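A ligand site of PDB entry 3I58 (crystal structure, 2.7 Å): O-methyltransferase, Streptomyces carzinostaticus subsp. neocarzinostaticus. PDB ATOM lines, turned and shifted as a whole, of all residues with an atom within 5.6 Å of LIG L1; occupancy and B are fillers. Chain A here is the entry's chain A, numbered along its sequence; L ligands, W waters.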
ATOM      1  N   TRP A 133     -29.163  -4.741   5.290  1.00  0.00           N
ATOM      2  CA  TRP A 133     -28.527  -5.931   4.718  1.00  0.00           C
ATOM      3  C   TRP A 133     -28.499  -5.908   3.205  1.00  0.00           C
ATOM      4  O   TRP A 133     -27.534  -6.373   2.589  1.00  0.00           O
ATOM      5  CB  TRP A 133     -29.244  -7.190   5.218  1.00  0.00           C
ATOM      6  CG  TRP A 133     -29.182  -7.340   6.710  1.00  0.00           C
ATOM      7  CD1 TRP A 133     -30.228  -7.556   7.557  1.00  0.00           C
ATOM      8  CD2 TRP A 133     -28.013  -7.259   7.542  1.00  0.00           C
ATOM      9  NE1 TRP A 133     -29.794  -7.604   8.859  1.00  0.00           N
ATOM     10  CE2 TRP A 133     -28.437  -7.422   8.876  1.00  0.00           C
ATOM     11  CE3 TRP A 133     -26.657  -7.053   7.283  1.00  0.00           C
ATOM     12  CZ2 TRP A 133     -27.541  -7.385   9.948  1.00  0.00           C
ATOM     13  CZ3 TRP A 133     -25.768  -7.016   8.348  1.00  0.00           C
ATOM     14  CH2 TRP A 133     -26.209  -7.190   9.672  1.00  0.00           C
ATOM     15  N   PHE A 146     -18.402  -2.906   7.833  1.00  0.00           N
ATOM     16  CA  PHE A 146     -19.252  -3.452   8.881  1.00  0.00           C
ATOM     17  C   PHE A 146     -18.535  -4.642   9.543  1.00  0.00           C
ATOM     18  O   PHE A 146     -18.519  -4.749  10.765  1.00  0.00           O
ATOM     19  CB  PHE A 146     -20.619  -3.867   8.322  1.00  0.00           C
ATOM     20  CG  PHE A 146     -21.628  -4.200   9.392  1.00  0.00           C
ATOM     21  CD1 PHE A 146     -21.972  -3.257  10.355  1.00  0.00           C
ATOM     22  CD2 PHE A 146     -22.163  -5.473   9.485  1.00  0.00           C
ATOM     23  CE1 PHE A 146     -22.827  -3.573  11.399  1.00  0.00           C
ATOM     24  CE2 PHE A 146     -23.028  -5.798  10.525  1.00  0.00           C
ATOM     25  CZ  PHE A 146     -23.362  -4.845  11.492  1.00  0.00           C
ATOM     26  N   ASP A 147     -17.932  -5.510   8.735  1.00  0.00           N
ATOM     27  CA  ASP A 147     -17.211  -6.685   9.255  1.00  0.00           C
ATOM     28  C   ASP A 147     -16.115  -6.275  10.248  1.00  0.00           C
ATOM     29  O   ASP A 147     -15.929  -6.903  11.281  1.00  0.00           O
ATOM     30  CB  ASP A 147     -16.565  -7.481   8.104  1.00  0.00           C
ATOM     31  CG  ASP A 147     -17.591  -8.185   7.242  1.00  0.00           C
ATOM     32  OD1 ASP A 147     -18.553  -8.726   7.825  1.00  0.00           O
ATOM     33  OD2 ASP A 147     -17.442  -8.222   5.989  1.00  0.00           O
ATOM     34  N   MET A 150     -17.777  -4.955  13.626  1.00  0.00           N
ATOM     35  CA  MET A 150     -18.255  -5.997  14.527  1.00  0.00           C
ATOM     36  C   MET A 150     -17.063  -6.733  15.096  1.00  0.00           C
ATOM     37  O   MET A 150     -17.091  -7.224  16.218  1.00  0.00           O
ATOM     38  CB  MET A 150     -19.170  -6.972  13.794  1.00  0.00           C
ATOM     39  CG  MET A 150     -20.476  -6.356  13.287  1.00  0.00           C
ATOM     40  SD  MET A 150     -21.455  -5.679  14.627  1.00  0.00           S
ATOM     41  CE  MET A 150     -21.017  -3.968  14.458  1.00  0.00           C
ATOM     42  N   SER A 151     -15.999  -6.801  14.301  1.00  0.00           N
ATOM     43  CA  SER A 151     -14.800  -7.474  14.751  1.00  0.00           C
ATOM     44  C   SER A 151     -14.267  -6.713  15.965  1.00  0.00           C
ATOM     45  O   SER A 151     -13.866  -7.306  16.964  1.00  0.00           O
ATOM     46  CB  SER A 151     -13.757  -7.508  13.629  1.00  0.00           C
ATOM     47  OG  SER A 151     -12.660  -8.312  13.988  1.00  0.00           O
ATOM     48  N   HIS A 153     -16.040  -4.706  17.945  1.00  0.00           N
ATOM     49  CA  HIS A 153     -17.005  -4.822  19.031  1.00  0.00           C
ATOM     50  C   HIS A 153     -16.684  -6.051  19.906  1.00  0.00           C
ATOM     51  O   HIS A 153     -16.943  -6.046  21.119  1.00  0.00           O
ATOM     52  CB  HIS A 153     -18.432  -4.875  18.449  1.00  0.00           C
ATOM     53  CG  HIS A 153     -19.189  -6.140  18.735  1.00  0.00           C
ATOM     54  ND1 HIS A 153     -19.827  -6.375  19.923  1.00  0.00           N
ATOM     55  CD2 HIS A 153     -19.429  -7.230  17.962  1.00  0.00           C
ATOM     56  CE1 HIS A 153     -20.422  -7.555  19.882  1.00  0.00           C
ATOM     57  NE2 HIS A 153     -20.195  -8.092  18.700  1.00  0.00           N
ATOM     58  N   LEU A 154     -16.113  -7.088  19.311  1.00  0.00           N
ATOM     59  CA  LEU A 154     -15.752  -8.302  20.032  1.00  0.00           C
ATOM     60  C   LEU A 154     -14.685  -8.016  21.094  1.00  0.00           C
ATOM     61  O   LEU A 154     -14.795  -8.487  22.234  1.00  0.00           O
ATOM     62  CB  LEU A 154     -15.200  -9.359  19.063  1.00  0.00           C
ATOM     63  CG  LEU A 154     -16.090  -9.902  17.945  1.00  0.00           C
ATOM     64  CD1 LEU A 154     -15.229 -10.671  16.973  1.00  0.00           C
ATOM     65  CD2 LEU A 154     -17.186 -10.790  18.514  1.00  0.00           C
ATOM     66  N   TYR A 158     -16.534  -8.660  24.410  1.00  0.00           N
ATOM     67  CA  TYR A 158     -16.350 -10.072  24.765  1.00  0.00           C
ATOM     68  C   TYR A 158     -15.076 -10.424  25.496  1.00  0.00           C
ATOM     69  O   TYR A 158     -14.682 -11.585  25.552  1.00  0.00           O
ATOM     70  CB  TYR A 158     -16.494 -10.938  23.505  1.00  0.00           C
ATOM     71  CG  TYR A 158     -17.865 -10.835  22.836  1.00  0.00           C
ATOM     72  CD1 TYR A 158     -18.982 -10.437  23.570  1.00  0.00           C
ATOM     73  CD2 TYR A 158     -18.048 -11.187  21.506  1.00  0.00           C
ATOM     74  CE1 TYR A 158     -20.232 -10.396  22.993  1.00  0.00           C
ATOM     75  CE2 TYR A 158     -19.305 -11.147  20.923  1.00  0.00           C
ATOM     76  CZ  TYR A 158     -20.385 -10.750  21.676  1.00  0.00           C
ATOM     77  OH  TYR A 158     -21.650 -10.719  21.131  1.00  0.00           O
ATOM     78  N   ASP A 175     -21.051 -20.985  14.465  1.00  0.00           N
ATOM     79  CA  ASP A 175     -21.303 -19.579  14.767  1.00  0.00           C
ATOM     80  C   ASP A 175     -22.262 -19.058  13.697  1.00  0.00           C
ATOM     81  O   ASP A 175     -21.836 -18.649  12.625  1.00  0.00           O
ATOM     82  CB  ASP A 175     -19.987 -18.791  14.744  1.00  0.00           C
ATOM     83  CG  ASP A 175     -20.081 -17.452  15.509  1.00  0.00           C
ATOM     84  OD1 ASP A 175     -21.061 -17.281  16.278  1.00  0.00           O
ATOM     85  OD2 ASP A 175     -19.187 -16.584  15.371  1.00  0.00           O
ATOM     86  N   VAL A 176     -23.557 -19.112  14.016  1.00  0.00           N
ATOM     87  CA  VAL A 176     -24.624 -18.663  13.119  1.00  0.00           C
ATOM     88  C   VAL A 176     -24.596 -17.141  13.018  1.00  0.00           C
ATOM     89  O   VAL A 176     -24.916 -16.444  13.981  1.00  0.00           O
ATOM     90  CB  VAL A 176     -26.008 -19.098  13.648  1.00  0.00           C
ATOM     91  CG1 VAL A 176     -27.081 -18.764  12.626  1.00  0.00           C
ATOM     92  CG2 VAL A 176     -26.010 -20.598  13.931  1.00  0.00           C
ATOM     93  N   GLY A 177     -24.208 -16.645  11.848  1.00  0.00           N
ATOM     94  CA  GLY A 177     -24.107 -15.213  11.653  1.00  0.00           C
ATOM     95  C   GLY A 177     -22.787 -14.708  12.201  1.00  0.00           C
ATOM     96  O   GLY A 177     -22.665 -13.543  12.573  1.00  0.00           O
ATOM     97  N   GLY A 178     -21.777 -15.591  12.237  1.00  0.00           N
ATOM     98  CA  GLY A 178     -20.469 -15.254  12.776  1.00  0.00           C
ATOM     99  C   GLY A 178     -19.545 -14.262  12.081  1.00  0.00           C
ATOM    100  O   GLY A 178     -18.365 -14.203  12.428  1.00  0.00           O
ATOM    101  N   GLY A 179     -20.032 -13.488  11.112  1.00  0.00           N
ATOM    102  CA  GLY A 179     -19.161 -12.517  10.462  1.00  0.00           C
ATOM    103  C   GLY A 179     -17.792 -12.971   9.975  1.00  0.00           C
ATOM    104  O   GLY A 179     -17.635 -14.078   9.462  1.00  0.00           O
ATOM    105  N   LEU A 199     -21.208 -19.532   9.745  1.00  0.00           N
ATOM    106  CA  LEU A 199     -22.314 -19.525   8.776  1.00  0.00           C
ATOM    107  C   LEU A 199     -22.716 -18.052   8.623  1.00  0.00           C
ATOM    108  O   LEU A 199     -23.031 -17.411   9.614  1.00  0.00           O
ATOM    109  CB  LEU A 199     -23.478 -20.351   9.329  1.00  0.00           C
ATOM    110  CG  LEU A 199     -24.759 -20.525   8.507  1.00  0.00           C
ATOM    111  CD1 LEU A 199     -25.566 -19.231   8.463  1.00  0.00           C
ATOM    112  CD2 LEU A 199     -24.387 -20.977   7.108  1.00  0.00           C
ATOM    113  N   ASP A 200     -22.690 -17.520   7.411  1.00  0.00           N
ATOM    114  CA  ASP A 200     -23.041 -16.109   7.218  1.00  0.00           C
ATOM    115  C   ASP A 200     -23.250 -15.834   5.738  1.00  0.00           C
ATOM    116  O   ASP A 200     -23.039 -16.707   4.909  1.00  0.00           O
ATOM    117  CB  ASP A 200     -21.904 -15.214   7.761  1.00  0.00           C
ATOM    118  CG  ASP A 200     -22.394 -13.864   8.325  1.00  0.00           C
ATOM    119  OD1 ASP A 200     -22.893 -13.013   7.565  1.00  0.00           O
ATOM    120  OD2 ASP A 200     -22.267 -13.664   9.557  1.00  0.00           O
ATOM    121  N   LEU A 201     -23.682 -14.622   5.403  1.00  0.00           N
ATOM    122  CA  LEU A 201     -23.868 -14.279   4.000  1.00  0.00           C
ATOM    123  C   LEU A 201     -22.485 -14.336   3.357  1.00  0.00           C
ATOM    124  O   LEU A 201     -21.470 -14.352   4.066  1.00  0.00           O
ATOM    125  CB  LEU A 201     -24.463 -12.879   3.875  1.00  0.00           C
ATOM    126  CG  LEU A 201     -25.782 -12.667   4.636  1.00  0.00           C
ATOM    127  CD1 LEU A 201     -26.230 -11.214   4.492  1.00  0.00           C
ATOM    128  CD2 LEU A 201     -26.835 -13.616   4.105  1.00  0.00           C
ATOM    129  N   PRO A 204     -19.214 -11.583   4.625  1.00  0.00           N
ATOM    130  CA  PRO A 204     -18.512 -11.908   5.860  1.00  0.00           C
ATOM    131  C   PRO A 204     -17.882 -13.316   5.824  1.00  0.00           C
ATOM    132  O   PRO A 204     -16.753 -13.498   6.256  1.00  0.00           O
ATOM    133  CB  PRO A 204     -19.611 -11.817   6.923  1.00  0.00           C
ATOM    134  CG  PRO A 204     -20.568 -10.837   6.333  1.00  0.00           C
ATOM    135  CD  PRO A 204     -20.618 -11.224   4.883  1.00  0.00           C
ATOM    136  N   GLY A 226     -24.547 -19.002   3.635  1.00  0.00           N
ATOM    137  CA  GLY A 226     -25.977 -19.278   3.691  1.00  0.00           C
ATOM    138  C   GLY A 226     -26.750 -18.393   4.649  1.00  0.00           C
ATOM    139  O   GLY A 226     -26.178 -17.716   5.485  1.00  0.00           O
ATOM    140  N   SER A 227     -28.067 -18.379   4.486  1.00  0.00           N
ATOM    141  CA  SER A 227     -28.935 -17.586   5.343  1.00  0.00           C
ATOM    142  C   SER A 227     -29.329 -18.414   6.564  1.00  0.00           C
ATOM    143  O   SER A 227     -29.612 -19.604   6.425  1.00  0.00           O
ATOM    144  CB  SER A 227     -30.197 -17.202   4.581  1.00  0.00           C
ATOM    145  OG  SER A 227     -31.226 -16.831   5.474  1.00  0.00           O
ATOM    146  N   PHE A 228     -29.319 -17.812   7.761  1.00  0.00           N
ATOM    147  CA  PHE A 228     -29.699 -18.567   8.950  1.00  0.00           C
ATOM    148  C   PHE A 228     -31.213 -18.696   9.065  1.00  0.00           C
ATOM    149  O   PHE A 228     -31.746 -19.062  10.107  1.00  0.00           O
ATOM    150  CB  PHE A 228     -29.111 -17.943  10.243  1.00  0.00           C
ATOM    151  CG  PHE A 228     -29.216 -16.442  10.327  1.00  0.00           C
ATOM    152  CD1 PHE A 228     -30.400 -15.793   9.998  1.00  0.00           C
ATOM    153  CD2 PHE A 228     -28.134 -15.693  10.757  1.00  0.00           C
ATOM    154  CE1 PHE A 228     -30.500 -14.416  10.097  1.00  0.00           C
ATOM    155  CE2 PHE A 228     -28.232 -14.306  10.853  1.00  0.00           C
ATOM    156  CZ  PHE A 228     -29.404 -13.669  10.526  1.00  0.00           C
ATOM    157  N   PHE A 229     -31.916 -18.373   7.984  1.00  0.00           N
ATOM    158  CA  PHE A 229     -33.361 -18.529   7.961  1.00  0.00           C
ATOM    159  C   PHE A 229     -33.663 -19.892   7.347  1.00  0.00           C
ATOM    160  O   PHE A 229     -34.738 -20.449   7.542  1.00  0.00           O
ATOM    161  CB  PHE A 229     -34.031 -17.402   7.171  1.00  0.00           C
ATOM    162  CG  PHE A 229     -34.115 -16.126   7.943  1.00  0.00           C
ATOM    163  CD1 PHE A 229     -33.363 -15.011   7.562  1.00  0.00           C
ATOM    164  CD2 PHE A 229     -34.942 -16.020   9.058  1.00  0.00           C
ATOM    165  CE1 PHE A 229     -33.430 -13.824   8.288  1.00  0.00           C
ATOM    166  CE2 PHE A 229     -35.017 -14.839   9.793  1.00  0.00           C
ATOM    167  CZ  PHE A 229     -34.261 -13.736   9.408  1.00  0.00           C
ATOM    168  N   SER A 242     -24.252 -14.721  18.112  1.00  0.00           N
ATOM    169  CA  SER A 242     -23.562 -13.574  18.700  1.00  0.00           C
ATOM    170  C   SER A 242     -23.958 -12.238  18.105  1.00  0.00           C
ATOM    171  O   SER A 242     -23.579 -11.906  16.983  1.00  0.00           O
ATOM    172  CB  SER A 242     -22.062 -13.800  18.541  1.00  0.00           C
ATOM    173  OG  SER A 242     -21.323 -12.654  18.920  1.00  0.00           O
ATOM    174  N   ALA A 243     -24.716 -11.455  18.882  1.00  0.00           N
ATOM    175  CA  ALA A 243     -25.179 -10.125  18.455  1.00  0.00           C
ATOM    176  C   ALA A 243     -25.974 -10.227  17.163  1.00  0.00           C
ATOM    177  O   ALA A 243     -25.784  -9.432  16.238  1.00  0.00           O
ATOM    178  CB  ALA A 243     -23.983  -9.184  18.288  1.00  0.00           C
ATOM    179  N   VAL A 244     -26.875 -11.202  17.130  1.00  0.00           N
ATOM    180  CA  VAL A 244     -27.729 -11.447  15.973  1.00  0.00           C
ATOM    181  C   VAL A 244     -29.188 -11.159  16.282  1.00  0.00           C
ATOM    182  O   VAL A 244     -29.839 -10.362  15.607  1.00  0.00           O
ATOM    183  CB  VAL A 244     -27.606 -12.919  15.486  1.00  0.00           C
ATOM    184  CG1 VAL A 244     -28.671 -13.227  14.422  1.00  0.00           C
ATOM    185  CG2 VAL A 244     -26.203 -13.186  14.936  1.00  0.00           C
ATOM    186  N   ASP A 247     -30.890  -7.822  16.108  1.00  0.00           N
ATOM    187  CA  ASP A 247     -30.999  -7.185  14.802  1.00  0.00           C
ATOM    188  C   ASP A 247     -32.358  -7.505  14.169  1.00  0.00           C
ATOM    189  O   ASP A 247     -32.664  -6.967  13.109  1.00  0.00           O
ATOM    190  CB  ASP A 247     -29.927  -7.687  13.835  1.00  0.00           C
ATOM    191  CG  ASP A 247     -28.526  -7.332  14.266  1.00  0.00           C
ATOM    192  OD1 ASP A 247     -28.365  -6.391  15.061  1.00  0.00           O
ATOM    193  OD2 ASP A 247     -27.565  -7.993  13.785  1.00  0.00           O
ATOM    194  N   TRP A 248     -33.144  -8.369  14.806  1.00  0.00           N
ATOM    195  CA  TRP A 248     -34.420  -8.800  14.251  1.00  0.00           C
ATOM    196  C   TRP A 248     -35.634  -8.635  15.152  1.00  0.00           C
ATOM    197  O   TRP A 248     -35.522  -8.729  16.370  1.00  0.00           O
ATOM    198  CB  TRP A 248     -34.345 -10.272  13.849  1.00  0.00           C
ATOM    199  CG  TRP A 248     -33.231 -10.574  12.917  1.00  0.00           C
ATOM    200  CD1 TRP A 248     -31.945 -10.891  13.265  1.00  0.00           C
ATOM    201  CD2 TRP A 248     -33.251 -10.444  11.499  1.00  0.00           C
ATOM    202  NE1 TRP A 248     -31.171 -10.971  12.134  1.00  0.00           N
ATOM    203  CE2 TRP A 248     -31.936 -10.704  11.035  1.00  0.00           C
ATOM    204  CE3 TRP A 248     -34.254 -10.142  10.566  1.00  0.00           C
ATOM    205  CZ2 TRP A 248     -31.608 -10.654   9.679  1.00  0.00           C
ATOM    206  CZ3 TRP A 248     -33.919 -10.092   9.217  1.00  0.00           C
ATOM    207  CH2 TRP A 248     -32.604 -10.354   8.783  1.00  0.00           C
HETATM  208  N1  LIG L   1     -21.249 -12.852  15.412  1.00  0.00           N
HETATM  209  C1  LIG L   1     -20.991 -11.529  14.827  1.00  0.00           C
HETATM  210  C2  LIG L   1     -22.327 -10.872  14.459  1.00  0.00           C
HETATM  211  C3  LIG L   1     -22.100  -9.673  13.535  1.00  0.00           C
HETATM  212  S1  LIG L   1     -23.614  -8.715  13.190  1.00  0.00           S
HETATM  213  C4  LIG L   1     -20.234 -10.646  15.823  1.00  0.00           C
HETATM  214  O1  LIG L   1     -19.325  -9.925  15.370  1.00  0.00           O
HETATM  215  O2  LIG L   1     -20.584 -10.701  17.022  1.00  0.00           O
HETATM  216  C5  LIG L   1     -24.795  -9.966  12.576  1.00  0.00           C
HETATM  217  C6  LIG L   1     -24.276 -10.911  11.488  1.00  0.00           C
HETATM  218  O3  LIG L   1     -25.411 -11.565  10.901  1.00  0.00           O
HETATM  219  C7  LIG L   1     -23.559 -10.176  10.340  1.00  0.00           C
HETATM  220  O4  LIG L   1     -22.364 -10.885  10.003  1.00  0.00           O
HETATM  221  C8  LIG L   1     -24.567 -10.287   9.187  1.00  0.00           C
HETATM  222  O5  LIG L   1     -23.869 -10.361   7.944  1.00  0.00           O
HETATM  223  C9  LIG L   1     -25.123 -11.675   9.507  1.00  0.00           C
HETATM  224  N2  LIG L   1     -26.361 -11.939   8.732  1.00  0.00           N
HETATM  225  C10 LIG L   1     -27.324 -11.054   8.458  1.00  0.00           C
HETATM  226  N3  LIG L   1     -28.327 -11.657   7.840  1.00  0.00           N
HETATM  227  C11 LIG L   1     -28.009 -12.946   7.714  1.00  0.00           C
HETATM  228  C12 LIG L   1     -28.662 -14.069   7.205  1.00  0.00           C
HETATM  229  N4  LIG L   1     -29.882 -13.963   6.697  1.00  0.00           N
HETATM  230  N5  LIG L   1     -28.050 -15.257   7.270  1.00  0.00           N
HETATM  231  C13 LIG L   1     -26.848 -15.386   7.800  1.00  0.00           C
HETATM  232  N6  LIG L   1     -26.198 -14.349   8.301  1.00  0.00           N
HETATM  233  C14 LIG L   1     -26.758 -13.126   8.281  1.00  0.00           C
HETATM  234  C1  LG2 L   2     -23.645  -5.489  18.816  1.00  0.00           C
HETATM  235  C2  LG2 L   2     -25.628  -2.480  14.131  1.00  0.00           C
HETATM  236  O1  LG2 L   2     -21.998  -2.214  19.475  1.00  0.00           O
HETATM  237  O2  LG2 L   2     -21.428  -0.085  19.470  1.00  0.00           O
HETATM  238  O3  LG2 L   2     -22.522   1.528  17.943  1.00  0.00           O
HETATM  239  C3  LG2 L   2     -23.854   0.715  16.156  1.00  0.00           C
HETATM  240  C4  LG2 L   2     -24.446  -0.356  15.483  1.00  0.00           C
HETATM  241  C5  LG2 L   2     -24.750  -4.011  15.782  1.00  0.00           C
HETATM  242  C6  LG2 L   2     -23.377  -3.172  17.581  1.00  0.00           C
HETATM  243  O4  LG2 L   2     -23.858  -5.501  17.399  1.00  0.00           O
HETATM  244  C7  LG2 L   2     -22.057  -1.055  19.002  1.00  0.00           C
HETATM  245  C8  LG2 L   2     -24.890  -2.716  15.291  1.00  0.00           C
HETATM  246  C9  LG2 L   2     -23.996  -4.234  16.922  1.00  0.00           C
HETATM  247  C10 LG2 L   2     -23.095   0.480  17.292  1.00  0.00           C
HETATM  248  C11 LG2 L   2     -22.926  -0.814  17.765  1.00  0.00           C
HETATM  249  C12 LG2 L   2     -24.278  -1.651  15.956  1.00  0.00           C
HETATM  250  C13 LG2 L   2     -23.525  -1.883  17.099  1.00  0.00           C
HETATM  251  O   HOH W   1     -25.574  -6.858  15.180  1.00  0.00           O
HETATM  252  O   HOH W   2     -20.216  -9.339  10.101  1.00  0.00           O
HETATM  253  O   HOH W   3     -23.322  -8.577   6.229  1.00  0.00           O
HETATM  254  O   HOH W   4     -23.085 -15.427  15.535  1.00  0.00           O
HETATM  255  O   HOH W   5     -19.378 -14.198  16.461  1.00  0.00           O
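An oxygen (O4) of LIG L1 lies within hydrogen-bond range of the side-chain carboxylate (OD2) of Asp 200 (2.8 Å).
The backbone carbonyl oxygen (O) of Ser 242 sits at hydrogen-bond distance from a nitrogen (N1) of LIG L1.
An oxygen (O2) of LIG L1 lies within hydrogen-bond range of the side-chain hydroxyl (OG) of Ser 242, at 2.8 Å.
N of Phe 228 is in hydrogen-bond range of N5 of LIG L1, at 2.9 Å.
A ring nitrogen (NE2) of His 153 is in hydrogen-bond range of an oxygen (O2) of LIG L1.
OG of Ser 227 is in hydrogen-bond range of N4 of LIG L1.
A nitrogen (N1) of LIG L1 sits at hydrogen-bond distance from the backbone carbonyl oxygen of Gly 177.
The backbone carbonyl oxygen (O) of Asp 200 sits at hydrogen-bond distance from the backbone NH (N) of Gly 226 (3.0 Å).
The side-chain carboxylate (OD2) of Asp 200 is in hydrogen-bond range of the backbone NH (N) of Gly 179 (2.7 Å).
The side-chain carboxylate of Asp 200 sits at hydrogen-bond distance from the backbone NH of Gly 178 (3.3 Å).
OG of Ser 242 sits at hydrogen-bond distance from OH of Tyr 158.
The side-chain hydroxyl (OG) of Ser 227 sits close to the backbone NH (N) of Phe 229, 3.0 Å away.
N of Gly 177 sits at hydrogen-bond distance from O of Leu 199 (2.6 Å).
The backbone carbonyl oxygen of Leu 199 sits at hydrogen-bond distance from the backbone NH of Gly 178.
Merely in contact with LIG L1: Met 150 (3.4 Å), Gly 226 (3.4 Å), Trp 133 (3.5 Å), Asp 247 (3.6 Å), Gly 179 (3.6 Å), Leu 201 (3.6 Å), Gly 178 (3.7 Å), Pro 204 (3.7 Å), Leu 154 (3.7 Å), Phe 229 (3.7 Å), Ala 243 (3.8 Å), Trp 248 (3.9 Å) and Phe 146 (3.99 Å).
Hydrophobic or aromatic side chains that line LIG L1: Trp 133, Phe 146, Met 150, His 153, Leu 154, Leu 201, Pro 204, Phe 228, Phe 229, Ala 243 and Trp 248.
19 residues have an atom within 4 Å of LIG L1: Trp 133, Phe 146, Met 150, His 153, Leu 154, Gly 177, Gly 178, Gly 179, Asp 200, Leu 201, Pro 204, Gly 226, Ser 227, Phe 228, Phe 229, Ser 242, Ala 243, Asp 247 and Trp 248.
Water W5 lies within hydrogen-bond range of N1 of LIG L1 (2.5 Å), OD2 of Asp 175 (2.6 Å) and OG of Ser 242 (3.5 Å).
Water W2 lies within hydrogen-bond range of an oxygen (O4) of LIG L1 (2.6 Å) and the side-chain carboxylate (OD1) of Asp 147 (2.9 Å).
Water W4 lies within hydrogen-bond range of the backbone carbonyl oxygen (O) of Val 176 (2.6 Å), the side-chain carboxylate (OD1) of Asp 175 (2.8 Å), the backbone NH (N) of Ser 242 (2.9 Å) and a nitrogen (N1) of LIG L1 (3.2 Å).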
